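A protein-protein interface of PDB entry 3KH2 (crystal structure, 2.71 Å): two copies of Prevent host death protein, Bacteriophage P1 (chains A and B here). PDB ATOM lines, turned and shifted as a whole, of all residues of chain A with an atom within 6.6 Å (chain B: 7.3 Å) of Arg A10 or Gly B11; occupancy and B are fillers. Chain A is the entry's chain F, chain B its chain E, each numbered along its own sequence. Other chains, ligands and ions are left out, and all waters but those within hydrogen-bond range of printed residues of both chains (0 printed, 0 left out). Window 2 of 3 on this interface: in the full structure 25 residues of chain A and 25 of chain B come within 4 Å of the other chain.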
ATOM      1  N   ILE A   4     -18.124  10.276 -26.335  1.00  0.00           N
ATOM      2  CA  ILE A   4     -18.860  10.735 -27.512  1.00  0.00           C
ATOM      3  C   ILE A   4     -18.891  12.256 -27.555  1.00  0.00           C
ATOM      4  O   ILE A   4     -18.745  12.920 -26.530  1.00  0.00           O
ATOM      5  CB  ILE A   4     -20.310  10.196 -27.543  1.00  0.00           C
ATOM      6  CG1 ILE A   4     -21.083  10.608 -26.287  1.00  0.00           C
ATOM      7  CG2 ILE A   4     -20.310   8.683 -27.680  1.00  0.00           C
ATOM      8  CD1 ILE A   4     -22.532  10.170 -26.293  1.00  0.00           C
ATOM      9  N   ASN A   5     -19.088  12.797 -28.751  1.00  0.00           N
ATOM     10  CA  ASN A   5     -19.126  14.239 -28.952  1.00  0.00           C
ATOM     11  C   ASN A   5     -20.512  14.834 -28.700  1.00  0.00           C
ATOM     12  O   ASN A   5     -21.535  14.234 -29.026  1.00  0.00           O
ATOM     13  CB  ASN A   5     -18.666  14.591 -30.374  1.00  0.00           C
ATOM     14  CG  ASN A   5     -18.605  16.093 -30.620  1.00  0.00           C
ATOM     15  OD1 ASN A   5     -18.349  16.879 -29.708  1.00  0.00           O
ATOM     16  ND2 ASN A   5     -18.836  16.496 -31.863  1.00  0.00           N
ATOM     17  N   PHE A   6     -20.507  16.007 -28.079  1.00  0.00           N
ATOM     18  CA  PHE A   6     -21.609  16.970 -28.102  1.00  0.00           C
ATOM     19  C   PHE A   6     -22.760  16.618 -29.063  1.00  0.00           C
ATOM     20  O   PHE A   6     -23.891  16.399 -28.622  1.00  0.00           O
ATOM     21  CB  PHE A   6     -20.971  18.321 -28.454  1.00  0.00           C
ATOM     22  CG  PHE A   6     -21.924  19.472 -28.568  1.00  0.00           C
ATOM     23  CD1 PHE A   6     -22.156  20.313 -27.488  1.00  0.00           C
ATOM     24  CD2 PHE A   6     -22.520  19.768 -29.781  1.00  0.00           C
ATOM     25  CE1 PHE A   6     -23.010  21.402 -27.606  1.00  0.00           C
ATOM     26  CE2 PHE A   6     -23.372  20.848 -29.908  1.00  0.00           C
ATOM     27  CZ  PHE A   6     -23.618  21.669 -28.820  1.00  0.00           C
ATOM     28  N   ARG A   7     -22.459  16.545 -30.360  1.00  0.00           N
ATOM     29  CA  ARG A   7     -23.474  16.310 -31.400  1.00  0.00           C
ATOM     30  C   ARG A   7     -24.064  14.906 -31.369  1.00  0.00           C
ATOM     31  O   ARG A   7     -25.283  14.739 -31.428  1.00  0.00           O
ATOM     32  CB  ARG A   7     -22.882  16.549 -32.789  1.00  0.00           C
ATOM     33  CG  ARG A   7     -22.503  17.984 -33.075  1.00  0.00           C
ATOM     34  CD  ARG A   7     -22.093  18.154 -34.530  1.00  0.00           C
ATOM     35  NE  ARG A   7     -21.703  19.529 -34.839  1.00  0.00           N
ATOM     36  CZ  ARG A   7     -20.460  20.010 -34.789  1.00  0.00           C
ATOM     37  NH1 ARG A   7     -19.433  19.242 -34.438  1.00  0.00           N
ATOM     38  NH2 ARG A   7     -20.241  21.284 -35.097  1.00  0.00           N
ATOM     39  N   THR A   8     -23.192  13.903 -31.305  1.00  0.00           N
ATOM     40  CA  THR A   8     -23.607  12.494 -31.281  1.00  0.00           C
ATOM     41  C   THR A   8     -24.580  12.210 -30.133  1.00  0.00           C
ATOM     42  O   THR A   8     -25.513  11.415 -30.277  1.00  0.00           O
ATOM     43  CB  THR A   8     -22.391  11.541 -31.146  1.00  0.00           C
ATOM     44  OG1 THR A   8     -21.245  12.114 -31.788  1.00  0.00           O
ATOM     45  CG2 THR A   8     -22.695  10.182 -31.760  1.00  0.00           C
ATOM     46  N   ALA A   9     -24.346  12.866 -28.997  1.00  0.00           N
ATOM     47  CA  ALA A   9     -25.227  12.767 -27.836  1.00  0.00           C
ATOM     48  C   ALA A   9     -26.604  13.337 -28.156  1.00  0.00           C
ATOM     49  O   ALA A   9     -27.621  12.682 -27.938  1.00  0.00           O
ATOM     50  CB  ALA A   9     -24.621  13.503 -26.652  1.00  0.00           C
ATOM     51  N   ARG A  10     -26.617  14.555 -28.686  1.00  0.00           N
ATOM     52  CA  ARG A  10     -27.858  15.241 -29.059  1.00  0.00           C
ATOM     53  C   ARG A  10     -28.763  14.349 -29.910  1.00  0.00           C
ATOM     54  O   ARG A  10     -29.966  14.262 -29.668  1.00  0.00           O
ATOM     55  CB  ARG A  10     -27.548  16.530 -29.830  1.00  0.00           C
ATOM     56  CG  ARG A  10     -28.455  17.697 -29.486  1.00  0.00           C
ATOM     57  CD  ARG A  10     -28.124  18.919 -30.336  1.00  0.00           C
ATOM     58  NE  ARG A  10     -28.519  20.174 -29.694  1.00  0.00           N
ATOM     59  CZ  ARG A  10     -28.269  21.390 -30.181  1.00  0.00           C
ATOM     60  NH1 ARG A  10     -27.621  21.544 -31.332  1.00  0.00           N
ATOM     61  NH2 ARG A  10     -28.672  22.465 -29.510  1.00  0.00           N
ATOM     62  N   GLY A  11     -28.168  13.686 -30.898  1.00  0.00           N
ATOM     63  CA  GLY A  11     -28.910  12.854 -31.848  1.00  0.00           C
ATOM     64  C   GLY A  11     -29.238  11.454 -31.360  1.00  0.00           C
ATOM     65  O   GLY A  11     -30.229  10.863 -31.791  1.00  0.00           O
ATOM     66  N   ASN A  12     -28.401  10.916 -30.474  1.00  0.00           N
ATOM     67  CA  ASN A  12     -28.585   9.557 -29.958  1.00  0.00           C
ATOM     68  C   ASN A  12     -28.694   9.535 -28.438  1.00  0.00           C
ATOM     69  O   ASN A  12     -28.178   8.629 -27.786  1.00  0.00           O
ATOM     70  CB  ASN A  12     -27.425   8.662 -30.404  1.00  0.00           C
ATOM     71  CG  ASN A  12     -27.184   8.719 -31.898  1.00  0.00           C
ATOM     72  OD1 ASN A  12     -28.122   8.812 -32.687  1.00  0.00           O
ATOM     73  ND2 ASN A  12     -25.919   8.659 -32.295  1.00  0.00           N
ATOM     74  N   LEU A  13     -29.383  10.523 -27.875  1.00  0.00           N
ATOM     75  CA  LEU A  13     -29.458  10.655 -26.423  1.00  0.00           C
ATOM     76  C   LEU A  13     -30.167   9.458 -25.808  1.00  0.00           C
ATOM     77  O   LEU A  13     -29.693   8.892 -24.829  1.00  0.00           O
ATOM     78  CB  LEU A  13     -30.164  11.953 -26.023  1.00  0.00           C
ATOM     79  CG  LEU A  13     -30.025  12.370 -24.553  1.00  0.00           C
ATOM     80  CD1 LEU A  13     -28.568  12.467 -24.135  1.00  0.00           C
ATOM     81  CD2 LEU A  13     -30.730  13.694 -24.307  1.00  0.00           C
ATOM     82  N   SER A  14     -31.290   9.067 -26.403  1.00  0.00           N
ATOM     83  CA  SER A  14     -32.068   7.923 -25.926  1.00  0.00           C
ATOM     84  C   SER A  14     -31.260   6.621 -25.899  1.00  0.00           C
ATOM     85  O   SER A  14     -31.546   5.732 -25.097  1.00  0.00           O
ATOM     86  CB  SER A  14     -33.319   7.738 -26.789  1.00  0.00           C
ATOM     87  OG  SER A  14     -32.974   7.625 -28.158  1.00  0.00           O
ATOM     88  N   PHE B   6     -35.570  14.403 -20.803  1.00  0.00           N
ATOM     89  CA  PHE B   6     -34.548  14.259 -21.849  1.00  0.00           C
ATOM     90  C   PHE B   6     -34.799  15.112 -23.102  1.00  0.00           C
ATOM     91  O   PHE B   6     -33.894  15.298 -23.915  1.00  0.00           O
ATOM     92  CB  PHE B   6     -34.337  12.774 -22.205  1.00  0.00           C
ATOM     93  CG  PHE B   6     -35.223  12.259 -23.314  1.00  0.00           C
ATOM     94  CD1 PHE B   6     -34.666  11.787 -24.498  1.00  0.00           C
ATOM     95  CD2 PHE B   6     -36.603  12.218 -23.168  1.00  0.00           C
ATOM     96  CE1 PHE B   6     -35.466  11.297 -25.524  1.00  0.00           C
ATOM     97  CE2 PHE B   6     -37.413  11.729 -24.195  1.00  0.00           C
ATOM     98  CZ  PHE B   6     -36.840  11.269 -25.372  1.00  0.00           C
ATOM     99  N   ARG B   7     -36.016  15.639 -23.242  1.00  0.00           N
ATOM    100  CA  ARG B   7     -36.354  16.551 -24.339  1.00  0.00           C
ATOM    101  C   ARG B   7     -35.816  17.962 -24.107  1.00  0.00           C
ATOM    102  O   ARG B   7     -35.217  18.554 -25.004  1.00  0.00           O
ATOM    103  CB  ARG B   7     -37.869  16.595 -24.554  1.00  0.00           C
ATOM    104  CG  ARG B   7     -38.402  15.381 -25.293  1.00  0.00           C
ATOM    105  CD  ARG B   7     -39.903  15.263 -25.179  1.00  0.00           C
ATOM    106  NE  ARG B   7     -40.402  14.125 -25.952  1.00  0.00           N
ATOM    107  CZ  ARG B   7     -41.333  13.263 -25.545  1.00  0.00           C
ATOM    108  NH1 ARG B   7     -41.889  13.364 -24.340  1.00  0.00           N
ATOM    109  NH2 ARG B   7     -41.702  12.271 -26.348  1.00  0.00           N
ATOM    110  N   THR B   8     -36.038  18.499 -22.909  1.00  0.00           N
ATOM    111  CA  THR B   8     -35.502  19.817 -22.543  1.00  0.00           C
ATOM    112  C   THR B   8     -33.971  19.826 -22.566  1.00  0.00           C
ATOM    113  O   THR B   8     -33.355  20.869 -22.789  1.00  0.00           O
ATOM    114  CB  THR B   8     -36.001  20.282 -21.151  1.00  0.00           C
ATOM    115  OG1 THR B   8     -36.087  19.160 -20.266  1.00  0.00           O
ATOM    116  CG2 THR B   8     -37.371  20.938 -21.262  1.00  0.00           C
ATOM    117  N   ALA B   9     -33.373  18.660 -22.336  1.00  0.00           N
ATOM    118  CA  ALA B   9     -31.929  18.479 -22.474  1.00  0.00           C
ATOM    119  C   ALA B   9     -31.496  18.587 -23.936  1.00  0.00           C
ATOM    120  O   ALA B   9     -30.558  19.319 -24.255  1.00  0.00           O
ATOM    121  CB  ALA B   9     -31.509  17.131 -21.900  1.00  0.00           C
ATOM    122  N   ARG B  10     -32.185  17.854 -24.809  1.00  0.00           N
ATOM    123  CA  ARG B  10     -31.884  17.840 -26.252  1.00  0.00           C
ATOM    124  C   ARG B  10     -31.771  19.236 -26.857  1.00  0.00           C
ATOM    125  O   ARG B  10     -30.807  19.542 -27.558  1.00  0.00           O
ATOM    126  CB  ARG B  10     -32.934  17.029 -27.031  1.00  0.00           C
ATOM    127  CG  ARG B  10     -32.445  15.661 -27.477  1.00  0.00           C
ATOM    128  CD  ARG B  10     -33.511  14.886 -28.238  1.00  0.00           C
ATOM    129  NE  ARG B  10     -32.996  13.605 -28.728  1.00  0.00           N
ATOM    130  CZ  ARG B  10     -33.716  12.693 -29.380  1.00  0.00           C
ATOM    131  NH1 ARG B  10     -35.004  12.900 -29.636  1.00  0.00           N
ATOM    132  NH2 ARG B  10     -33.142  11.563 -29.779  1.00  0.00           N
ATOM    133  N   GLY B  11     -32.764  20.075 -26.580  1.00  0.00           N
ATOM    134  CA  GLY B  11     -32.804  21.433 -27.117  1.00  0.00           C
ATOM    135  C   GLY B  11     -31.834  22.390 -26.450  1.00  0.00           C
ATOM    136  O   GLY B  11     -31.327  23.313 -27.088  1.00  0.00           O
ATOM    137  N   ASN B  12     -31.574  22.170 -25.164  1.00  0.00           N
ATOM    138  CA  ASN B  12     -30.752  23.080 -24.369  1.00  0.00           C
ATOM    139  C   ASN B  12     -29.501  22.405 -23.812  1.00  0.00           C
ATOM    140  O   ASN B  12     -29.127  22.631 -22.660  1.00  0.00           O
ATOM    141  CB  ASN B  12     -31.587  23.654 -23.223  1.00  0.00           C
ATOM    142  CG  ASN B  12     -32.964  24.095 -23.670  1.00  0.00           C
ATOM    143  OD1 ASN B  12     -33.118  24.722 -24.717  1.00  0.00           O
ATOM    144  ND2 ASN B  12     -33.976  23.763 -22.881  1.00  0.00           N
ATOM    145  N   LEU B  13     -28.849  21.588 -24.635  1.00  0.00           N
ATOM    146  CA  LEU B  13     -27.664  20.850 -24.197  1.00  0.00           C
ATOM    147  C   LEU B  13     -26.513  21.790 -23.838  1.00  0.00           C
ATOM    148  O   LEU B  13     -25.833  21.577 -22.839  1.00  0.00           O
ATOM    149  CB  LEU B  13     -27.212  19.847 -25.265  1.00  0.00           C
ATOM    150  CG  LEU B  13     -26.086  18.886 -24.860  1.00  0.00           C
ATOM    151  CD1 LEU B  13     -26.472  18.073 -23.636  1.00  0.00           C
ATOM    152  CD2 LEU B  13     -25.727  17.966 -26.016  1.00  0.00           C
ATOM    153  N   SER B  14     -26.309  22.829 -24.644  1.00  0.00           N
ATOM    154  CA  SER B  14     -25.224  23.791 -24.408  1.00  0.00           C
ATOM    155  C   SER B  14     -25.404  24.585 -23.108  1.00  0.00           C
ATOM    156  O   SER B  14     -24.422  25.017 -22.503  1.00  0.00           O
ATOM    157  CB  SER B  14     -25.073  24.745 -25.600  1.00  0.00           C
ATOM    158  OG  SER B  14     -26.197  25.596 -25.737  1.00  0.00           O
ATOM    159  N   GLU B  15     -26.655  24.776 -22.690  1.00  0.00           N
ATOM    160  CA  GLU B  15     -26.953  25.390 -21.394  1.00  0.00           C
ATOM    161  C   GLU B  15     -26.564  24.449 -20.254  1.00  0.00           C
ATOM    162  O   GLU B  15     -25.941  24.867 -19.275  1.00  0.00           O
ATOM    163  CB  GLU B  15     -28.440  25.744 -21.280  1.00  0.00           C
ATOM    164  CG  GLU B  15     -28.897  26.882 -22.184  1.00  0.00           C
ATOM    165  CD  GLU B  15     -30.368  27.243 -21.994  1.00  0.00           C
ATOM    166  OE1 GLU B  15     -31.047  26.617 -21.152  1.00  0.00           O
ATOM    167  OE2 GLU B  15     -30.849  28.160 -22.693  1.00  0.00           O
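The guanidinium group (NE) of Arg A10 sits at hydrogen-bond distance from the backbone carbonyl oxygen (O) of Arg B10.
Phe A6 touches Leu B13, and with the chains exchanged Leu A13 touches Phe B6. Arg A10 touches its own counterpart, Arg B10. Arg A10 touches Gly B11, and with the chains exchanged Gly A11 touches Arg B10.
Phe A6 touches Leu B13. Gly B11 touches Arg A10 (O to NH2, 3.7 Å). NH2 of Arg B10 touches O of Gly A11, 3.6 Å away. CD2 of Leu A13 touches O of Phe B6 (3.6 Å).
Of the 11 printed residues of chain A, 4 touch a printed residue of chain B. Hydrophobic or aromatic side chains of chain A that line the printed part of chain B: Leu A13. Hydrophobic or aromatic side chains of chain B that line the printed part of chain A: Leu B13. Among the printed residues, no Asp or Glu carboxylate lies within 4 Å of a Lys or Arg side-chain nitrogen of the other chain.
Of chain B, only Arg B10 and Gly B11 come within 4 Å of Arg A10. Gly B11 touches one residue of chain A. No residue of chain B comes within 4 Å of Ala A9. Printed residues of chain B within 4 Å of Leu A13: Phe B6. Of the printed residues of chain A, Leu B13 touches Phe A6. Of the printed residues of chain A, Phe B6 touches Leu A13 (3.6 Å). Of the printed residues of chain B, Gly A11 touches Arg B10 (3.6 Å). Asn A12 touches none of the printed residues of chain B. Thr B8 touches none of the printed residues of chain A. The nearest residue of chain B that does not touch Arg A10 is Leu B13 (4.4 Å). The nearest printed residue of chain A that does not touch Gly B11 is Leu A13 (7.1 Å).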
